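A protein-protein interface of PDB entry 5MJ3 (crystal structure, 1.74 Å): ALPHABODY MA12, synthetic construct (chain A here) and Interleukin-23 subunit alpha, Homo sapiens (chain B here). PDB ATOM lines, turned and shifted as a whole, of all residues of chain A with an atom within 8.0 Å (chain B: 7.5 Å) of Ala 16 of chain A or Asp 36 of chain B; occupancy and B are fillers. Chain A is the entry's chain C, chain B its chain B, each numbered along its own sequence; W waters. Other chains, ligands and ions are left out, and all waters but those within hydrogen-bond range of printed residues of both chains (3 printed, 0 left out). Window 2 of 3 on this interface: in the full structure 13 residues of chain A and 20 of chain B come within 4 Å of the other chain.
O of Leu 37 of chain B sits at hydrogen-bond distance from NH2 of Arg 148 of chain B (3.3 Å).
The guanidinium group (NH1) of Arg 148 of chain B lies within hydrogen-bond range of the backbone carbonyl oxygen (O) of Asp 36 of chain B.
The side-chain carboxylate of Asp 36 of chain B is in hydrogen-bond range of the backbone NH of Gly 33 of chain B.
Among the printed residues, pairs that only touch across the chains: Gln 13 of chain A with Leu 37 of chain B (3.6 Å), Gln 13 of chain A with Leu 141 of chain B (3.5 Å), Ala 16 of chain A with Val 32 of chain B (3.7 Å), Ala 16 of chain A with Asp 36 of chain B (3.4 Å), Val 17 of chain A with Leu 141 of chain B (3.9 Å), Val 17 of chain A with Phe 144 of chain B (3.9 Å), Gly 20 of chain A with Pro 30 of chain B (3.9 Å) and Gly 20 of chain A with Leu 31 of chain B (3.0 Å).
Of the printed residues of chain B, Ala 16 of chain A touches Val 32 and Asp 36.
Asp 36 of chain B touches one residue of chain A.
Gly 33 of chain B touches none of the printed residues of chain A.
Of the printed residues of chain A, Val 32 of chain B touches Ala 16 (3.7 Å).
Of the printed residues of chain A, Leu 31 of chain B touches Gly 20.
Of the printed residues of chain A, Pro 30 of chain B touches Gly 20 (3.9 Å).
Asp 42 of chain B touches none of the printed residues of chain A.
Ile 106 of chain A touches none of the printed residues of chain B.
The nearest printed residue of chain B that does not touch Gln 13 of chain A is Glu 39 of chain B (4.6 Å).
Printed residues of chain B that touch a printed residue of chain A: Pro 30, Leu 31, Val 32, Asp 36, Leu 37, Leu 141 and Phe 144.
Hydrophobic or aromatic side chains of chain B within 4 Å of the printed part of chain A: Pro 30, Val 32, Leu 37, Leu 141 and Phe 144.
Of the 17 printed residues of chain A, 4 touch a printed residue of chain B.
Along chain A the printed residues that touch a printed residue of chain B span positions 13 to 20.
Among the printed residues, 8 pairs touch across the chains.
Among the printed residues, no Asp or Glu carboxylate lies within 4 Å of a Lys or Arg side-chain nitrogen of the other chain.
Water W1 lies within hydrogen-bond range of the side-chain amino group (NZ) of Lys 145 of chain B (2.7 Å) and the side-chain amide nitrogen (NE2) of Gln 13 of chain A (3.1 Å).
Water W2 bridges O of Gly 20 of chain A (2.8 Å) and N of Leu 31 of chain B (2.9 Å).
Water W3 lies within hydrogen-bond range of O of Ala 16 of chain A (2.9 Å), OD2 of Asp 36 of chain B (3.3 Å) and N of Gly 33 of chain B (3.4 Å).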
ATOM      1  N   LYS A   9      -1.086  18.895  -0.374  1.00  0.00           N
ATOM      2  CA  LYS A   9      -0.059  17.860  -0.325  1.00  0.00           C
ATOM      3  C   LYS A   9      -0.137  16.940  -1.536  1.00  0.00           C
ATOM      4  O   LYS A   9       0.893  16.582  -2.114  1.00  0.00           O
ATOM      5  CB  LYS A   9      -0.191  17.047   0.965  1.00  0.00           C
ATOM      6  CG  LYS A   9       0.855  15.952   1.126  1.00  0.00           C
ATOM      7  CD  LYS A   9       0.564  15.076   2.338  1.00  0.00           C
ATOM      8  N   GLU A  10      -1.345  16.511  -1.911  1.00  0.00           N
ATOM      9  CA  GLU A  10      -1.492  15.639  -3.073  1.00  0.00           C
ATOM     10  C   GLU A  10      -1.035  16.340  -4.339  1.00  0.00           C
ATOM     11  O   GLU A  10      -0.406  15.725  -5.209  1.00  0.00           O
ATOM     12  CB  GLU A  10      -2.945  15.193  -3.227  1.00  0.00           C
ATOM     13  CG  GLU A  10      -3.316  13.974  -2.418  1.00  0.00           C
ATOM     14  CD  GLU A  10      -4.766  13.573  -2.612  1.00  0.00           C
ATOM     15  OE1 GLU A  10      -5.618  14.473  -2.769  1.00  0.00           O
ATOM     16  OE2 GLU A  10      -5.051  12.357  -2.613  1.00  0.00           O
ATOM     17  N   ILE A  11      -1.345  17.632  -4.458  1.00  0.00           N
ATOM     18  CA  ILE A  11      -0.922  18.389  -5.630  1.00  0.00           C
ATOM     19  C   ILE A  11       0.590  18.498  -5.666  1.00  0.00           C
ATOM     20  O   ILE A  11       1.205  18.398  -6.731  1.00  0.00           O
ATOM     21  CB  ILE A  11      -1.574  19.779  -5.637  1.00  0.00           C
ATOM     22  CG1 ILE A  11      -3.063  19.622  -5.909  1.00  0.00           C
ATOM     23  CG2 ILE A  11      -0.941  20.677  -6.707  1.00  0.00           C
ATOM     24  CD1 ILE A  11      -3.838  20.827  -5.639  1.00  0.00           C
ATOM     25  N   ALA A  12       1.207  18.724  -4.512  1.00  0.00           N
ATOM     26  CA  ALA A  12       2.659  18.851  -4.471  1.00  0.00           C
ATOM     27  C   ALA A  12       3.326  17.552  -4.887  1.00  0.00           C
ATOM     28  O   ALA A  12       4.337  17.562  -5.602  1.00  0.00           O
ATOM     29  CB  ALA A  12       3.108  19.264  -3.071  1.00  0.00           C
ATOM     30  N   GLN A  13       2.765  16.439  -4.471  1.00  0.00           N
ATOM     31  CA  GLN A  13       3.314  15.158  -4.868  1.00  0.00           C
ATOM     32  C   GLN A  13       3.193  14.943  -6.367  1.00  0.00           C
ATOM     33  O   GLN A  13       4.102  14.530  -6.992  1.00  0.00           O
ATOM     34  CB  GLN A  13       2.700  14.008  -4.084  1.00  0.00           C
ATOM     35  CG  GLN A  13       2.940  14.110  -2.600  1.00  0.00           C
ATOM     36  CD  GLN A  13       2.462  12.927  -1.803  1.00  0.00           C
ATOM     37  OE1 GLN A  13       1.609  12.196  -2.225  1.00  0.00           O
ATOM     38  NE2 GLN A  13       2.996  12.781  -0.622  1.00  0.00           N
ATOM     39  N   ILE A  14       2.036  15.244  -6.871  1.00  0.00           N
ATOM     40  CA  ILE A  14       1.807  15.094  -8.294  1.00  0.00           C
ATOM     41  C   ILE A  14       2.771  16.033  -9.080  1.00  0.00           C
ATOM     42  O   ILE A  14       3.370  15.644 -10.055  1.00  0.00           O
ATOM     43  CB  ILE A  14       0.359  15.490  -8.761  1.00  0.00           C
ATOM     44  CG1 ILE A  14      -0.670  14.483  -8.244  1.00  0.00           C
ATOM     45  CG2 ILE A  14       0.318  15.726 -10.252  1.00  0.00           C
ATOM     46  CD1 ILE A  14      -2.101  14.875  -8.432  1.00  0.00           C
ATOM     47  N   GLN A  15       2.911  17.291  -8.658  1.00  0.00           N
ATOM     48  CA  GLN A  15       3.870  18.199  -9.339  1.00  0.00           C
ATOM     49  C   GLN A  15       5.301  17.557  -9.277  1.00  0.00           C
ATOM     50  O   GLN A  15       6.015  17.601 -10.229  1.00  0.00           O
ATOM     51  CB  GLN A  15       4.017  19.640  -8.690  1.00  0.00           C
ATOM     52  CG  GLN A  15       2.793  20.537  -8.779  1.00  0.00           C
ATOM     53  CD  GLN A  15       2.767  21.430 -10.057  1.00  0.00           C
ATOM     54  OE1 GLN A  15       3.013  20.930 -11.149  1.00  0.00           O
ATOM     55  NE2 GLN A  15       2.532  22.727  -9.911  1.00  0.00           N
ATOM     56  N   ALA A  16       5.718  17.031  -8.123  1.00  0.00           N
ATOM     57  CA  ALA A  16       7.082  16.425  -8.047  1.00  0.00           C
ATOM     58  C   ALA A  16       7.238  15.223  -9.033  1.00  0.00           C
ATOM     59  O   ALA A  16       8.189  15.097  -9.741  1.00  0.00           O
ATOM     60  CB  ALA A  16       7.487  15.949  -6.627  1.00  0.00           C
ATOM     61  N   VAL A  17       6.242  14.357  -9.064  1.00  0.00           N
ATOM     62  CA  VAL A  17       6.344  13.149  -9.881  1.00  0.00           C
ATOM     63  C   VAL A  17       6.397  13.508 -11.362  1.00  0.00           C
ATOM     64  O   VAL A  17       7.225  12.976 -12.113  1.00  0.00           O
ATOM     65  CB  VAL A  17       5.180  12.192  -9.566  1.00  0.00           C
ATOM     66  CG1 VAL A  17       5.106  11.054 -10.585  1.00  0.00           C
ATOM     67  CG2 VAL A  17       5.326  11.640  -8.157  1.00  0.00           C
ATOM     68  N   ILE A  18       5.522  14.411 -11.813  1.00  0.00           N
ATOM     69  CA  ILE A  18       5.533  14.724 -13.242  1.00  0.00           C
ATOM     70  C   ILE A  18       6.793  15.491 -13.632  1.00  0.00           C
ATOM     71  O   ILE A  18       7.313  15.296 -14.738  1.00  0.00           O
ATOM     72  CB  ILE A  18       4.257  15.477 -13.683  1.00  0.00           C
ATOM     73  CG1 ILE A  18       4.108  16.805 -12.941  1.00  0.00           C
ATOM     74  CG2 ILE A  18       3.049  14.577 -13.515  1.00  0.00           C
ATOM     75  CD1 ILE A  18       2.753  17.501 -13.158  1.00  0.00           C
ATOM     76  N   ALA A  19       7.316  16.353 -12.750  1.00  0.00           N
ATOM     77  CA  ALA A  19       8.596  17.000 -13.036  1.00  0.00           C
ATOM     78  C   ALA A  19       9.708  15.968 -13.184  1.00  0.00           C
ATOM     79  O   ALA A  19      10.591  16.114 -14.041  1.00  0.00           O
ATOM     80  CB  ALA A  19       8.955  18.004 -11.942  1.00  0.00           C
ATOM     81  N   GLY A  20       9.682  14.918 -12.355  1.00  0.00           N
ATOM     82  CA  GLY A  20      10.690  13.872 -12.456  1.00  0.00           C
ATOM     83  C   GLY A  20      10.555  13.046 -13.722  1.00  0.00           C
ATOM     84  O   GLY A  20      11.550  12.713 -14.370  1.00  0.00           O
ATOM     85  N   ILE A  21       9.323  12.711 -14.098  1.00  0.00           N
ATOM     86  CA  ILE A  21       9.109  11.997 -15.351  1.00  0.00           C
ATOM     87  C   ILE A  21       9.589  12.845 -16.519  1.00  0.00           C
ATOM     88  O   ILE A  21      10.251  12.350 -17.439  1.00  0.00           O
ATOM     89  CB  ILE A  21       7.623  11.602 -15.479  1.00  0.00           C
ATOM     90  CG1 ILE A  21       7.300  10.510 -14.444  1.00  0.00           C
ATOM     91  CG2 ILE A  21       7.293  11.124 -16.900  1.00  0.00           C
ATOM     92  CD1 ILE A  21       5.824  10.187 -14.290  1.00  0.00           C
ATOM     93  N   GLN A  22       9.294  14.143 -16.479  1.00  0.00           N
ATOM     94  CA  GLN A  22       9.735  15.059 -17.526  1.00  0.00           C
ATOM     95  C   GLN A  22      11.256  15.041 -17.673  1.00  0.00           C
ATOM     96  O   GLN A  22      11.784  14.979 -18.791  1.00  0.00           O
ATOM     97  CB  GLN A  22       9.234  16.461 -17.193  1.00  0.00           C
ATOM     98  CG  GLN A  22       9.142  17.429 -18.342  1.00  0.00           C
ATOM     99  CD  GLN A  22       8.369  18.684 -17.949  1.00  0.00           C
ATOM    100  OE1 GLN A  22       8.440  19.133 -16.803  1.00  0.00           O
ATOM    101  NE2 GLN A  22       7.614  19.238 -18.887  1.00  0.00           N
ATOM    102  N   LYS A  23      11.977  15.105 -16.551  1.00  0.00           N
ATOM    103  CA  LYS A  23      13.435  15.095 -16.604  1.00  0.00           C
ATOM    104  C   LYS A  23      13.955  13.751 -17.095  1.00  0.00           C
ATOM    105  O   LYS A  23      14.958  13.687 -17.818  1.00  0.00           O
ATOM    106  CB  LYS A  23      14.004  15.419 -15.227  1.00  0.00           C
ATOM    107  CG  LYS A  23      15.518  15.332 -15.132  1.00  0.00           C
ATOM    108  CD  LYS A  23      16.023  15.853 -13.792  1.00  0.00           C
ATOM    109  N   GLN A  59       0.695  19.477 -16.306  1.00  0.00           N
ATOM    110  CA  GLN A  59       1.270  20.539 -15.486  1.00  0.00           C
ATOM    111  C   GLN A  59       0.414  21.801 -15.609  1.00  0.00           C
ATOM    112  O   GLN A  59       0.180  22.517 -14.633  1.00  0.00           O
ATOM    113  CB  GLN A  59       2.715  20.829 -15.898  1.00  0.00           C
ATOM    114  CG  GLN A  59       3.685  19.711 -15.550  1.00  0.00           C
ATOM    115  CD  GLN A  59       5.091  19.978 -16.057  1.00  0.00           C
ATOM    116  OE1 GLN A  59       5.293  20.266 -17.240  1.00  0.00           O
ATOM    117  NE2 GLN A  59       6.071  19.883 -15.161  1.00  0.00           N
ATOM    118  N   ILE A 106      -1.085  10.081 -15.193  1.00  0.00           N
ATOM    119  CA  ILE A 106       0.343   9.965 -14.917  1.00  0.00           C
ATOM    120  C   ILE A 106       0.767   8.504 -14.930  1.00  0.00           C
ATOM    121  O   ILE A 106       1.835   8.154 -15.447  1.00  0.00           O
ATOM    122  CB  ILE A 106       0.694  10.642 -13.575  1.00  0.00           C
ATOM    123  CG1 ILE A 106       0.502  12.146 -13.711  1.00  0.00           C
ATOM    124  CG2 ILE A 106       2.131  10.356 -13.176  1.00  0.00           C
ATOM    125  CD1 ILE A 106       0.579  12.912 -12.387  1.00  0.00           C
ATOM    126  N   PRO B  30      12.773   7.393 -12.986  1.00  0.00           N
ATOM    127  CA  PRO B  30      12.594   8.819 -12.686  1.00  0.00           C
ATOM    128  C   PRO B  30      12.895   9.137 -11.227  1.00  0.00           C
ATOM    129  O   PRO B  30      12.780   8.287 -10.340  1.00  0.00           O
ATOM    130  CB  PRO B  30      11.118   9.070 -13.016  1.00  0.00           C
ATOM    131  CG  PRO B  30      10.769   8.051 -13.989  1.00  0.00           C
ATOM    132  CD  PRO B  30      11.592   6.836 -13.663  1.00  0.00           C
ATOM    133  N   LEU B  31      13.283  10.388 -10.993  1.00  0.00           N
ATOM    134  CA  LEU B  31      13.695  10.912  -9.695  1.00  0.00           C
ATOM    135  C   LEU B  31      12.743  12.026  -9.276  1.00  0.00           C
ATOM    136  O   LEU B  31      12.087  12.633 -10.117  1.00  0.00           O
ATOM    137  CB  LEU B  31      15.115  11.499  -9.755  1.00  0.00           C
ATOM    138  CG  LEU B  31      16.182  10.732 -10.551  1.00  0.00           C
ATOM    139  CD1 LEU B  31      17.387  11.597 -10.904  1.00  0.00           C
ATOM    140  CD2 LEU B  31      16.636   9.595  -9.720  1.00  0.00           C
ATOM    141  N   VAL B  32      12.691  12.323  -7.978  1.00  0.00           N
ATOM    142  CA  VAL B  32      12.082  13.563  -7.501  1.00  0.00           C
ATOM    143  C   VAL B  32      13.152  14.355  -6.746  1.00  0.00           C
ATOM    144  O   VAL B  32      14.258  13.874  -6.494  1.00  0.00           O
ATOM    145  CB  VAL B  32      10.838  13.331  -6.616  1.00  0.00           C
ATOM    146  CG1 VAL B  32       9.716  12.624  -7.386  1.00  0.00           C
ATOM    147  CG2 VAL B  32      11.180  12.553  -5.350  1.00  0.00           C
ATOM    148  N   GLY B  33      12.807  15.581  -6.371  1.00  0.00           N
ATOM    149  CA  GLY B  33      13.733  16.383  -5.592  1.00  0.00           C
ATOM    150  C   GLY B  33      13.885  15.841  -4.185  1.00  0.00           C
ATOM    151  O   GLY B  33      12.987  15.193  -3.649  1.00  0.00           O
ATOM    152  N   HIS B  34      15.039  16.131  -3.557  1.00  0.00           N
ATOM    153  CA  HIS B  34      15.291  15.593  -2.219  1.00  0.00           C
ATOM    154  C   HIS B  34      14.338  16.147  -1.165  1.00  0.00           C
ATOM    155  O   HIS B  34      14.158  15.516  -0.119  1.00  0.00           O
ATOM    156  CB  HIS B  34      16.746  15.829  -1.797  1.00  0.00           C
ATOM    157  CG  HIS B  34      17.085  17.247  -1.448  1.00  0.00           C
ATOM    158  ND1 HIS B  34      17.167  17.688  -0.145  1.00  0.00           N
ATOM    159  CD2 HIS B  34      17.431  18.301  -2.223  1.00  0.00           C
ATOM    160  CE1 HIS B  34      17.531  18.959  -0.131  1.00  0.00           C
ATOM    161  NE2 HIS B  34      17.697  19.355  -1.378  1.00  0.00           N
ATOM    162  N   MET B  35      13.705  17.286  -1.413  1.00  0.00           N
ATOM    163  CA  MET B  35      12.698  17.833  -0.516  1.00  0.00           C
ATOM    164  C   MET B  35      11.284  17.357  -0.833  1.00  0.00           C
ATOM    165  O   MET B  35      10.342  17.753  -0.139  1.00  0.00           O
ATOM    166  CB  MET B  35      12.738  19.361  -0.571  1.00  0.00           C
ATOM    167  CG  MET B  35      14.136  19.930  -0.351  1.00  0.00           C
ATOM    168  SD  MET B  35      14.758  19.697   1.330  1.00  0.00           S
ATOM    169  CE  MET B  35      13.670  20.793   2.240  1.00  0.00           C
ATOM    170  N   ASP B  36      11.111  16.533  -1.864  1.00  0.00           N
ATOM    171  CA  ASP B  36       9.796  16.067  -2.279  1.00  0.00           C
ATOM    172  C   ASP B  36       9.440  14.735  -1.621  1.00  0.00           C
ATOM    173  O   ASP B  36      10.311  13.955  -1.222  1.00  0.00           O
ATOM    174  CB  ASP B  36       9.736  15.902  -3.798  1.00  0.00           C
ATOM    175  CG  ASP B  36      10.014  17.190  -4.554  1.00  0.00           C
ATOM    176  OD1 ASP B  36       9.688  18.280  -4.050  1.00  0.00           O
ATOM    177  OD2 ASP B  36      10.534  17.101  -5.687  1.00  0.00           O
ATOM    178  N   LEU B  37       8.130  14.495  -1.524  1.00  0.00           N
ATOM    179  CA  LEU B  37       7.563  13.246  -1.011  1.00  0.00           C
ATOM    180  C   LEU B  37       8.041  12.933   0.406  1.00  0.00           C
ATOM    181  O   LEU B  37       8.229  11.770   0.775  1.00  0.00           O
ATOM    182  CB  LEU B  37       7.877  12.077  -1.954  1.00  0.00           C
ATOM    183  CG  LEU B  37       7.557  12.277  -3.436  1.00  0.00           C
ATOM    184  CD1 LEU B  37       7.828  10.984  -4.231  1.00  0.00           C
ATOM    185  CD2 LEU B  37       6.117  12.739  -3.635  1.00  0.00           C
ATOM    186  N   ARG B  38       8.221  13.971   1.214  1.00  0.00           N
ATOM    187  CA  ARG B  38       8.603  13.813   2.609  1.00  0.00           C
ATOM    188  C   ARG B  38       7.353  13.945   3.471  1.00  0.00           C
ATOM    189  O   ARG B  38       6.406  14.645   3.103  1.00  0.00           O
ATOM    190  CB  ARG B  38       9.641  14.862   3.022  1.00  0.00           C
ATOM    191  CG  ARG B  38      10.936  14.863   2.194  1.00  0.00           C
ATOM    192  CD  ARG B  38      11.839  13.658   2.480  1.00  0.00           C
ATOM    193  NE  ARG B  38      13.030  13.707   1.629  1.00  0.00           N
ATOM    194  CZ  ARG B  38      13.952  12.753   1.523  1.00  0.00           C
ATOM    195  NH1 ARG B  38      13.872  11.615   2.215  1.00  0.00           N
ATOM    196  NH2 ARG B  38      14.970  12.954   0.709  1.00  0.00           N
ATOM    197  N   GLU B  39       7.345  13.267   4.617  1.00  0.00           N
ATOM    198  CA  GLU B  39       6.188  13.348   5.505  1.00  0.00           C
ATOM    199  C   GLU B  39       6.605  13.009   6.931  1.00  0.00           C
ATOM    200  O   GLU B  39       7.704  12.510   7.180  1.00  0.00           O
ATOM    201  CB  GLU B  39       5.054  12.437   5.028  1.00  0.00           C
ATOM    202  CG  GLU B  39       5.479  11.026   4.711  1.00  0.00           C
ATOM    203  CD  GLU B  39       4.414  10.264   3.953  1.00  0.00           C
ATOM    204  OE1 GLU B  39       3.401  10.888   3.565  1.00  0.00           O
ATOM    205  OE2 GLU B  39       4.592   9.044   3.740  1.00  0.00           O
ATOM    206  N   ASP B  42       8.007   9.611   8.311  1.00  0.00           N
ATOM    207  CA  ASP B  42       9.200   9.053   7.683  1.00  0.00           C
ATOM    208  C   ASP B  42      10.214   8.576   8.714  1.00  0.00           C
ATOM    209  O   ASP B  42      11.005   7.671   8.430  1.00  0.00           O
ATOM    210  CB  ASP B  42       9.843  10.090   6.759  1.00  0.00           C
ATOM    211  CG  ASP B  42       9.121  10.224   5.429  1.00  0.00           C
ATOM    212  OD1 ASP B  42       8.441   9.263   5.011  1.00  0.00           O
ATOM    213  OD2 ASP B  42       9.246  11.292   4.795  1.00  0.00           O
ATOM    214  N   LEU B 141       4.796   6.015  -5.557  1.00  0.00           N
ATOM    215  CA  LEU B 141       5.470   6.923  -4.630  1.00  0.00           C
ATOM    216  C   LEU B 141       6.550   6.194  -3.846  1.00  0.00           C
ATOM    217  O   LEU B 141       7.655   6.725  -3.644  1.00  0.00           O
ATOM    218  CB  LEU B 141       4.466   7.557  -3.662  1.00  0.00           C
ATOM    219  CG  LEU B 141       3.410   8.481  -4.268  1.00  0.00           C
ATOM    220  CD1 LEU B 141       2.495   8.994  -3.155  1.00  0.00           C
ATOM    221  CD2 LEU B 141       4.039   9.645  -5.002  1.00  0.00           C
ATOM    222  N   PHE B 144       9.960   5.803  -5.624  1.00  0.00           N
ATOM    223  CA  PHE B 144      10.850   6.953  -5.528  1.00  0.00           C
ATOM    224  C   PHE B 144      11.589   6.954  -4.202  1.00  0.00           C
ATOM    225  O   PHE B 144      12.792   7.232  -4.155  1.00  0.00           O
ATOM    226  CB  PHE B 144      10.081   8.269  -5.674  1.00  0.00           C
ATOM    227  CG  PHE B 144       9.581   8.540  -7.048  1.00  0.00           C
ATOM    228  CD1 PHE B 144      10.446   8.978  -8.033  1.00  0.00           C
ATOM    229  CD2 PHE B 144       8.234   8.406  -7.348  1.00  0.00           C
ATOM    230  CE1 PHE B 144       9.989   9.260  -9.304  1.00  0.00           C
ATOM    231  CE2 PHE B 144       7.767   8.663  -8.636  1.00  0.00           C
ATOM    232  CZ  PHE B 144       8.640   9.089  -9.611  1.00  0.00           C
ATOM    233  N   LYS B 145      10.875   6.669  -3.112  1.00  0.00           N
ATOM    234  CA  LYS B 145      11.483   6.717  -1.786  1.00  0.00           C
ATOM    235  C   LYS B 145      12.507   5.616  -1.599  1.00  0.00           C
ATOM    236  O   LYS B 145      13.564   5.835  -0.995  1.00  0.00           O
ATOM    237  CB  LYS B 145      10.399   6.619  -0.712  1.00  0.00           C
ATOM    238  CG  LYS B 145       9.366   7.730  -0.784  1.00  0.00           C
ATOM    239  CD  LYS B 145       8.284   7.513   0.279  1.00  0.00           C
ATOM    240  CE  LYS B 145       7.206   8.571   0.214  1.00  0.00           C
ATOM    241  NZ  LYS B 145       6.199   8.416   1.322  1.00  0.00           N
ATOM    242  N   ARG B 148      15.795   6.384  -3.736  1.00  0.00           N
ATOM    243  CA  ARG B 148      16.703   7.415  -3.239  1.00  0.00           C
ATOM    244  C   ARG B 148      17.419   6.961  -1.980  1.00  0.00           C
ATOM    245  O   ARG B 148      18.561   7.374  -1.734  1.00  0.00           O
ATOM    246  CB  ARG B 148      15.975   8.744  -3.034  1.00  0.00           C
ATOM    247  CG  ARG B 148      14.897   8.766  -2.005  1.00  0.00           C
ATOM    248  CD  ARG B 148      14.335  10.175  -1.965  1.00  0.00           C
ATOM    249  NE  ARG B 148      13.220  10.310  -1.053  1.00  0.00           N
ATOM    250  CZ  ARG B 148      12.384  11.341  -1.056  1.00  0.00           C
ATOM    251  NH1 ARG B 148      12.512  12.295  -1.954  1.00  0.00           N
ATOM    252  NH2 ARG B 148      11.392  11.398  -0.183  1.00  0.00           N
HETATM  253  O   HOH W   1       4.585  10.213   0.091  1.00  0.00           O
HETATM  254  O   HOH W   2      13.986  12.224 -13.094  1.00  0.00           O
HETATM  255  O   HOH W   3      10.720  16.367  -8.927  1.00  0.00           O
